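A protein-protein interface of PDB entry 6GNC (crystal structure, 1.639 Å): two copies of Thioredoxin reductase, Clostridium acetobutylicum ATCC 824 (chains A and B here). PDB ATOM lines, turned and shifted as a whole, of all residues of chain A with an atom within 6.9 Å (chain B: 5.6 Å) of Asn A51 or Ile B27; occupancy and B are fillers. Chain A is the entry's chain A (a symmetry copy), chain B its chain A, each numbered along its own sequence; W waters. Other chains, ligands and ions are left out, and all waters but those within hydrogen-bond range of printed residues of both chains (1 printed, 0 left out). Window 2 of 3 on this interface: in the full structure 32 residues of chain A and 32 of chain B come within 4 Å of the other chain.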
ATOM      1  N   LYS A  49     -11.656 -17.663  -5.960  1.00  0.00           N
ATOM      2  CA  LYS A  49     -12.241 -16.954  -7.102  1.00  0.00           C
ATOM      3  C   LYS A  49     -13.587 -16.427  -6.648  1.00  0.00           C
ATOM      4  O   LYS A  49     -14.321 -17.138  -5.974  1.00  0.00           O
ATOM      5  CB  LYS A  49     -12.415 -17.884  -8.300  1.00  0.00           C
ATOM      6  CG  LYS A  49     -11.154 -18.086  -9.115  1.00  0.00           C
ATOM      7  CD  LYS A  49     -10.732 -16.805  -9.809  1.00  0.00           C
ATOM      8  CE  LYS A  49      -9.576 -17.051 -10.759  1.00  0.00           C
ATOM      9  NZ  LYS A  49      -9.200 -15.818 -11.500  1.00  0.00           N
ATOM     10  N   ILE A  50     -13.948 -15.218  -7.051  1.00  0.00           N
ATOM     11  CA  ILE A  50     -15.193 -14.634  -6.557  1.00  0.00           C
ATOM     12  C   ILE A  50     -15.941 -14.089  -7.758  1.00  0.00           C
ATOM     13  O   ILE A  50     -15.440 -13.187  -8.439  1.00  0.00           O
ATOM     14  CB  ILE A  50     -14.937 -13.517  -5.528  1.00  0.00           C
ATOM     15  CG1 ILE A  50     -14.132 -14.055  -4.341  1.00  0.00           C
ATOM     16  CG2 ILE A  50     -16.262 -12.838  -5.139  1.00  0.00           C
ATOM     17  CD1 ILE A  50     -13.345 -12.957  -3.573  1.00  0.00           C
ATOM     18  N   ASN A  51     -17.138 -14.620  -8.021  1.00  0.00           N
ATOM     19  CA  ASN A  51     -17.931 -14.151  -9.152  1.00  0.00           C
ATOM     20  C   ASN A  51     -19.278 -13.594  -8.753  1.00  0.00           C
ATOM     21  O   ASN A  51     -20.103 -13.322  -9.636  1.00  0.00           O
ATOM     22  CB  ASN A  51     -18.137 -15.282 -10.152  1.00  0.00           C
ATOM     23  CG  ASN A  51     -16.903 -15.574 -10.935  1.00  0.00           C
ATOM     24  OD1 ASN A  51     -16.234 -14.659 -11.421  1.00  0.00           O
ATOM     25  ND2 ASN A  51     -16.550 -16.843 -11.017  1.00  0.00           N
ATOM     26  N   ASN A  52     -19.535 -13.505  -7.455  1.00  0.00           N
ATOM     27  CA  ASN A  52     -20.801 -12.965  -6.962  1.00  0.00           C
ATOM     28  C   ASN A  52     -20.801 -11.512  -6.413  1.00  0.00           C
ATOM     29  O   ASN A  52     -21.745 -11.146  -5.723  1.00  0.00           O
ATOM     30  CB  ASN A  52     -21.430 -13.915  -5.943  1.00  0.00           C
ATOM     31  CG  ASN A  52     -20.651 -13.986  -4.654  1.00  0.00           C
ATOM     32  OD1 ASN A  52     -19.519 -13.532  -4.578  1.00  0.00           O
ATOM     33  ND2 ASN A  52     -21.262 -14.559  -3.630  1.00  0.00           N
ATOM     34  N   TYR A  53     -19.767 -10.702  -6.657  1.00  0.00           N
ATOM     35  CA  TYR A  53     -19.765  -9.329  -6.198  1.00  0.00           C
ATOM     36  C   TYR A  53     -20.054  -8.552  -7.474  1.00  0.00           C
ATOM     37  O   TYR A  53     -19.197  -8.473  -8.336  1.00  0.00           O
ATOM     38  CB  TYR A  53     -18.383  -8.983  -5.650  1.00  0.00           C
ATOM     39  CG  TYR A  53     -18.317  -7.693  -4.879  1.00  0.00           C
ATOM     40  CD1 TYR A  53     -18.107  -6.490  -5.525  1.00  0.00           C
ATOM     41  CD2 TYR A  53     -18.452  -7.682  -3.502  1.00  0.00           C
ATOM     42  CE1 TYR A  53     -18.043  -5.308  -4.822  1.00  0.00           C
ATOM     43  CE2 TYR A  53     -18.389  -6.505  -2.790  1.00  0.00           C
ATOM     44  CZ  TYR A  53     -18.184  -5.322  -3.455  1.00  0.00           C
ATOM     45  OH  TYR A  53     -18.121  -4.149  -2.753  1.00  0.00           O
ATOM     46  N   LEU A  54     -21.211  -7.906  -7.572  1.00  0.00           N
ATOM     47  CA  LEU A  54     -21.578  -7.246  -8.815  1.00  0.00           C
ATOM     48  C   LEU A  54     -20.576  -6.163  -9.239  1.00  0.00           C
ATOM     49  O   LEU A  54     -20.237  -5.294  -8.452  1.00  0.00           O
ATOM     50  CB  LEU A  54     -22.963  -6.624  -8.671  1.00  0.00           C
ATOM     51  CG  LEU A  54     -23.489  -5.848  -9.876  1.00  0.00           C
ATOM     52  CD1 LEU A  54     -23.680  -6.772 -11.068  1.00  0.00           C
ATOM     53  CD2 LEU A  54     -24.790  -5.151  -9.522  1.00  0.00           C
ATOM     54  N   ILE A  56     -17.266  -6.538 -10.146  1.00  0.00           N
ATOM     55  CA  ILE A  56     -15.876  -6.955 -10.124  1.00  0.00           C
ATOM     56  C   ILE A  56     -15.953  -8.468 -10.228  1.00  0.00           C
ATOM     57  O   ILE A  56     -16.391  -9.115  -9.291  1.00  0.00           O
ATOM     58  CB  ILE A  56     -15.194  -6.556  -8.805  1.00  0.00           C
ATOM     59  CG1 ILE A  56     -15.426  -5.076  -8.518  1.00  0.00           C
ATOM     60  CG2 ILE A  56     -13.707  -6.857  -8.857  1.00  0.00           C
ATOM     61  CD1 ILE A  56     -14.856  -4.616  -7.198  1.00  0.00           C
ATOM     62  N   TYR A  57     -15.450  -9.058 -11.303  1.00  0.00           N
ATOM     63  CA  TYR A  57     -15.598 -10.494 -11.467  1.00  0.00           C
ATOM     64  C   TYR A  57     -14.311 -11.216 -11.800  1.00  0.00           C
ATOM     65  O   TYR A  57     -13.340 -10.618 -12.244  1.00  0.00           O
ATOM     66  CB  TYR A  57     -16.633 -10.781 -12.556  1.00  0.00           C
ATOM     67  CG  TYR A  57     -16.213 -10.309 -13.924  1.00  0.00           C
ATOM     68  CD1 TYR A  57     -15.463 -11.123 -14.754  1.00  0.00           C
ATOM     69  CD2 TYR A  57     -16.562  -9.051 -14.383  1.00  0.00           C
ATOM     70  CE1 TYR A  57     -15.072 -10.698 -16.005  1.00  0.00           C
ATOM     71  CE2 TYR A  57     -16.176  -8.618 -15.633  1.00  0.00           C
ATOM     72  CZ  TYR A  57     -15.429  -9.449 -16.438  1.00  0.00           C
ATOM     73  OH  TYR A  57     -15.037  -9.030 -17.684  1.00  0.00           O
ATOM     74  N   ASP A  58     -14.322 -12.516 -11.544  1.00  0.00           N
ATOM     75  CA  ASP A  58     -13.170 -13.390 -11.817  1.00  0.00           C
ATOM     76  C   ASP A  58     -11.933 -12.920 -11.062  1.00  0.00           C
ATOM     77  O   ASP A  58     -10.822 -12.874 -11.596  1.00  0.00           O
ATOM     78  CB  ASP A  58     -12.883 -13.507 -13.319  1.00  0.00           C
ATOM     79  CG  ASP A  58     -11.764 -14.524 -13.640  1.00  0.00           C
ATOM     80  OD1 ASP A  58     -11.692 -15.595 -12.993  1.00  0.00           O
ATOM     81  OD2 ASP A  58     -10.967 -14.255 -14.565  1.00  0.00           O
ATOM     82  N   VAL A  59     -12.131 -12.587  -9.795  1.00  0.00           N
ATOM     83  CA  VAL A  59     -11.043 -12.106  -8.956  1.00  0.00           C
ATOM     84  C   VAL A  59     -10.884 -13.032  -7.768  1.00  0.00           C
ATOM     85  O   VAL A  59     -11.855 -13.573  -7.235  1.00  0.00           O
ATOM     86  CB  VAL A  59     -11.285 -10.668  -8.457  1.00  0.00           C
ATOM     87  CG1 VAL A  59     -11.044  -9.676  -9.577  1.00  0.00           C
ATOM     88  CG2 VAL A  59     -12.687 -10.534  -7.864  1.00  0.00           C
ATOM     89  N   ALA B  22     -29.698 -12.010 -10.023  1.00  0.00           N
ATOM     90  CA  ALA B  22     -29.538 -12.948 -11.129  1.00  0.00           C
ATOM     91  C   ALA B  22     -28.194 -13.651 -11.070  1.00  0.00           C
ATOM     92  O   ALA B  22     -28.113 -14.868 -11.221  1.00  0.00           O
ATOM     93  CB  ALA B  22     -29.696 -12.211 -12.452  1.00  0.00           C
ATOM     94  N   ILE B  23     -27.123 -12.907 -10.788  1.00  0.00           N
ATOM     95  CA  ILE B  23     -25.808 -13.531 -10.739  1.00  0.00           C
ATOM     96  C   ILE B  23     -25.747 -14.563  -9.615  1.00  0.00           C
ATOM     97  O   ILE B  23     -25.226 -15.668  -9.801  1.00  0.00           O
ATOM     98  CB  ILE B  23     -24.743 -12.423 -10.589  1.00  0.00           C
ATOM     99  CG1 ILE B  23     -24.600 -11.650 -11.908  1.00  0.00           C
ATOM    100  CG2 ILE B  23     -23.432 -12.970 -10.142  1.00  0.00           C
ATOM    101  CD1 ILE B  23     -23.851 -10.338 -11.725  1.00  0.00           C
ATOM    102  N   ASN B  24     -26.307 -14.238  -8.447  1.00  0.00           N
ATOM    103  CA  ASN B  24     -26.214 -15.148  -7.319  1.00  0.00           C
ATOM    104  C   ASN B  24     -27.085 -16.385  -7.529  1.00  0.00           C
ATOM    105  O   ASN B  24     -26.692 -17.490  -7.146  1.00  0.00           O
ATOM    106  CB  ASN B  24     -26.592 -14.418  -6.043  1.00  0.00           C
ATOM    107  CG  ASN B  24     -25.407 -13.671  -5.455  1.00  0.00           C
ATOM    108  OD1 ASN B  24     -24.628 -14.261  -4.735  1.00  0.00           O
ATOM    109  ND2 ASN B  24     -25.233 -12.403  -5.837  1.00  0.00           N
ATOM    110  N   ALA B  25     -28.222 -16.224  -8.196  1.00  0.00           N
ATOM    111  CA  ALA B  25     -29.092 -17.371  -8.458  1.00  0.00           C
ATOM    112  C   ALA B  25     -28.472 -18.310  -9.482  1.00  0.00           C
ATOM    113  O   ALA B  25     -28.560 -19.534  -9.345  1.00  0.00           O
ATOM    114  CB  ALA B  25     -30.452 -16.873  -8.923  1.00  0.00           C
ATOM    115  N   VAL B  26     -27.827 -17.757 -10.501  1.00  0.00           N
ATOM    116  CA  VAL B  26     -27.175 -18.572 -11.528  1.00  0.00           C
ATOM    117  C   VAL B  26     -25.990 -19.331 -10.948  1.00  0.00           C
ATOM    118  O   VAL B  26     -25.755 -20.498 -11.288  1.00  0.00           O
ATOM    119  CB  VAL B  26     -26.783 -17.652 -12.696  1.00  0.00           C
ATOM    120  CG1 VAL B  26     -25.794 -18.302 -13.642  1.00  0.00           C
ATOM    121  CG2 VAL B  26     -28.069 -17.220 -13.409  1.00  0.00           C
ATOM    122  N   ILE B  27     -25.256 -18.669 -10.056  1.00  0.00           N
ATOM    123  CA  ILE B  27     -24.094 -19.263  -9.401  1.00  0.00           C
ATOM    124  C   ILE B  27     -24.563 -20.459  -8.599  1.00  0.00           C
ATOM    125  O   ILE B  27     -23.841 -21.433  -8.429  1.00  0.00           O
ATOM    126  CB  ILE B  27     -23.348 -18.264  -8.509  1.00  0.00           C
ATOM    127  CG1 ILE B  27     -22.544 -17.304  -9.379  1.00  0.00           C
ATOM    128  CG2 ILE B  27     -22.423 -19.001  -7.557  1.00  0.00           C
ATOM    129  CD1 ILE B  27     -21.773 -16.268  -8.598  1.00  0.00           C
ATOM    130  N   ARG B  28     -25.797 -20.382  -8.124  1.00  0.00           N
ATOM    131  CA  ARG B  28     -26.409 -21.484  -7.391  1.00  0.00           C
ATOM    132  C   ARG B  28     -27.149 -22.545  -8.264  1.00  0.00           C
ATOM    133  O   ARG B  28     -27.989 -23.256  -7.714  1.00  0.00           O
ATOM    134  CB  ARG B  28     -27.362 -20.960  -6.313  1.00  0.00           C
ATOM    135  CG  ARG B  28     -26.724 -20.028  -5.299  1.00  0.00           C
ATOM    136  CD  ARG B  28     -25.687 -20.739  -4.453  1.00  0.00           C
ATOM    137  NE  ARG B  28     -24.911 -19.799  -3.650  1.00  0.00           N
ATOM    138  CZ  ARG B  28     -25.029 -19.654  -2.335  1.00  0.00           C
ATOM    139  NH1 ARG B  28     -25.891 -20.398  -1.656  1.00  0.00           N
ATOM    140  NH2 ARG B  28     -24.275 -18.768  -1.699  1.00  0.00           N
ATOM    141  N   ASN B  29     -26.907 -22.602  -9.592  1.00  0.00           N
ATOM    142  CA  ASN B  29     -27.505 -23.549 -10.521  1.00  0.00           C
ATOM    143  C   ASN B  29     -29.011 -23.463 -10.684  1.00  0.00           C
ATOM    144  O   ASN B  29     -29.655 -24.469 -10.951  1.00  0.00           O
ATOM    145  CB  ASN B  29     -27.046 -24.988 -10.236  1.00  0.00           C
ATOM    146  CG  ASN B  29     -25.537 -25.111 -10.183  1.00  0.00           C
ATOM    147  OD1 ASN B  29     -24.984 -25.697  -9.253  1.00  0.00           O
ATOM    148  ND2 ASN B  29     -24.863 -24.545 -11.173  1.00  0.00           N
ATOM    149  N   HIS B  71     -19.908  -8.052 -16.340  1.00  0.00           N
ATOM    150  CA  HIS B  71     -20.093  -9.152 -15.388  1.00  0.00           C
ATOM    151  C   HIS B  71     -21.208 -10.082 -15.847  1.00  0.00           C
ATOM    152  O   HIS B  71     -21.050 -11.308 -15.857  1.00  0.00           O
ATOM    153  CB  HIS B  71     -20.430  -8.546 -14.021  1.00  0.00           C
ATOM    154  CG  HIS B  71     -20.246  -9.449 -12.835  1.00  0.00           C
ATOM    155  ND1 HIS B  71     -20.175 -10.826 -12.889  1.00  0.00           N
ATOM    156  CD2 HIS B  71     -20.172  -9.128 -11.522  1.00  0.00           C
ATOM    157  CE1 HIS B  71     -20.045 -11.305 -11.652  1.00  0.00           C
ATOM    158  NE2 HIS B  71     -20.017 -10.293 -10.816  1.00  0.00           N
ATOM    159  N   TYR B  74     -20.035 -12.170 -18.697  1.00  0.00           N
ATOM    160  CA  TYR B  74     -19.127 -13.203 -18.237  1.00  0.00           C
ATOM    161  C   TYR B  74     -19.913 -14.390 -17.688  1.00  0.00           C
ATOM    162  O   TYR B  74     -19.529 -15.548 -17.906  1.00  0.00           O
ATOM    163  CB  TYR B  74     -18.186 -12.620 -17.179  1.00  0.00           C
ATOM    164  CG  TYR B  74     -17.204 -13.629 -16.682  1.00  0.00           C
ATOM    165  CD1 TYR B  74     -16.191 -14.098 -17.501  1.00  0.00           C
ATOM    166  CD2 TYR B  74     -17.300 -14.136 -15.399  1.00  0.00           C
ATOM    167  CE1 TYR B  74     -15.298 -15.040 -17.054  1.00  0.00           C
ATOM    168  CE2 TYR B  74     -16.416 -15.077 -14.944  1.00  0.00           C
ATOM    169  CZ  TYR B  74     -15.413 -15.525 -15.774  1.00  0.00           C
ATOM    170  OH  TYR B  74     -14.517 -16.469 -15.327  1.00  0.00           O
ATOM    171  N   MET B  75     -21.024 -14.118 -17.007  1.00  0.00           N
ATOM    172  CA  MET B  75     -21.854 -15.148 -16.392  1.00  0.00           C
ATOM    173  C   MET B  75     -22.869 -15.729 -17.371  1.00  0.00           C
ATOM    174  O   MET B  75     -23.640 -16.615 -16.990  1.00  0.00           O
ATOM    175  CB  MET B  75     -22.583 -14.582 -15.164  1.00  0.00           C
ATOM    176  CG  MET B  75     -21.680 -14.074 -14.011  1.00  0.00           C
ATOM    177  SD  MET B  75     -20.534 -15.359 -13.475  1.00  0.00           S
ATOM    178  CE  MET B  75     -21.691 -16.468 -12.676  1.00  0.00           C
HETATM  179  O   HOH W   1     -14.188 -16.968 -12.849  1.00  0.00           O
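Among the printed residues, merely in contact across the chains: Asn A51 with Ile B23, Asn A52 with Asn B24, Asn A51 with Ile B27, Asn A51 with Tyr B74, Tyr A57 with His B71, Asn A52 with Ile B27, Leu A54 with His B71, Tyr A57 with Tyr B74, Leu A54 with Ile B23 and Asp A58 with Tyr B74.
No position is printed for both chains.
The side-chain carboxylate (OD1) of Asp A58 is in salt-bridge range of the side-chain amino group (NZ) of Lys A49 (2.9 Å). The backbone carbonyl oxygen of Ile A50 sits at hydrogen-bond distance from the backbone NH of Asp A58 (3.4 Å). The side-chain amide oxygen (OD1) of Asn A51 lies within hydrogen-bond range of the backbone NH (N) of Asp A58 (2.9 Å).
Of the 11 printed residues of chain B, 5 touch a printed residue of chain A. Printed residues of chain B that touch a printed residue of chain A: Ile B23, Asn B24, Ile B27, His B71 and Tyr B74. Hydrophobic or aromatic side chains of chain B that line the printed part of chain A: Ile B23, Ile B27, His B71 and Tyr B74. Of the 10 printed residues of chain A, 6 touch a printed residue of chain B. Hydrophobic or aromatic side chains of chain A that line the printed part of chain B: Leu A54 and Tyr A57. Among the printed residues, 12 pairs touch across the chains. Among the printed residues, no Asp or Glu carboxylate lies within 4 Å of a Lys or Arg side-chain nitrogen of the other chain.
NE2 of His B71 lies close to O of Asn A51 (3.3 Å). NE2 of His B71 sits at hydrogen-bond distance from O of Tyr A53, 3.2 Å away.
Of chain B, only Ile B23, Ile B27, His B71 and Tyr B74 come within 4 Å of Asn A51. Of the printed residues of chain B, Tyr A53 touches His B71. Printed residues of chain B within 4 Å of Leu A54: Ile B23 (3.6 Å) and His B71 (3.6 Å). Printed residues of chain B within 4 Å of Tyr A57: His B71 (3.6 Å) and Tyr B74 (3.6 Å). Ile B27 touches just these residues of chain A: Asn A51 (3.5 Å) and Asn A52 (3.6 Å). Of the printed residues of chain A, Tyr B74 touches Asn A51, Tyr A57 and Asp A58. The nearest residue of chain A that does not touch Ile B27 is Tyr A53 (6.2 Å).
Water W1 lies within hydrogen-bond range of OH of Tyr B74 (2.5 Å), OD1 of Asp A58 (2.9 Å) and ND2 of Asn A51 (3.0 Å).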
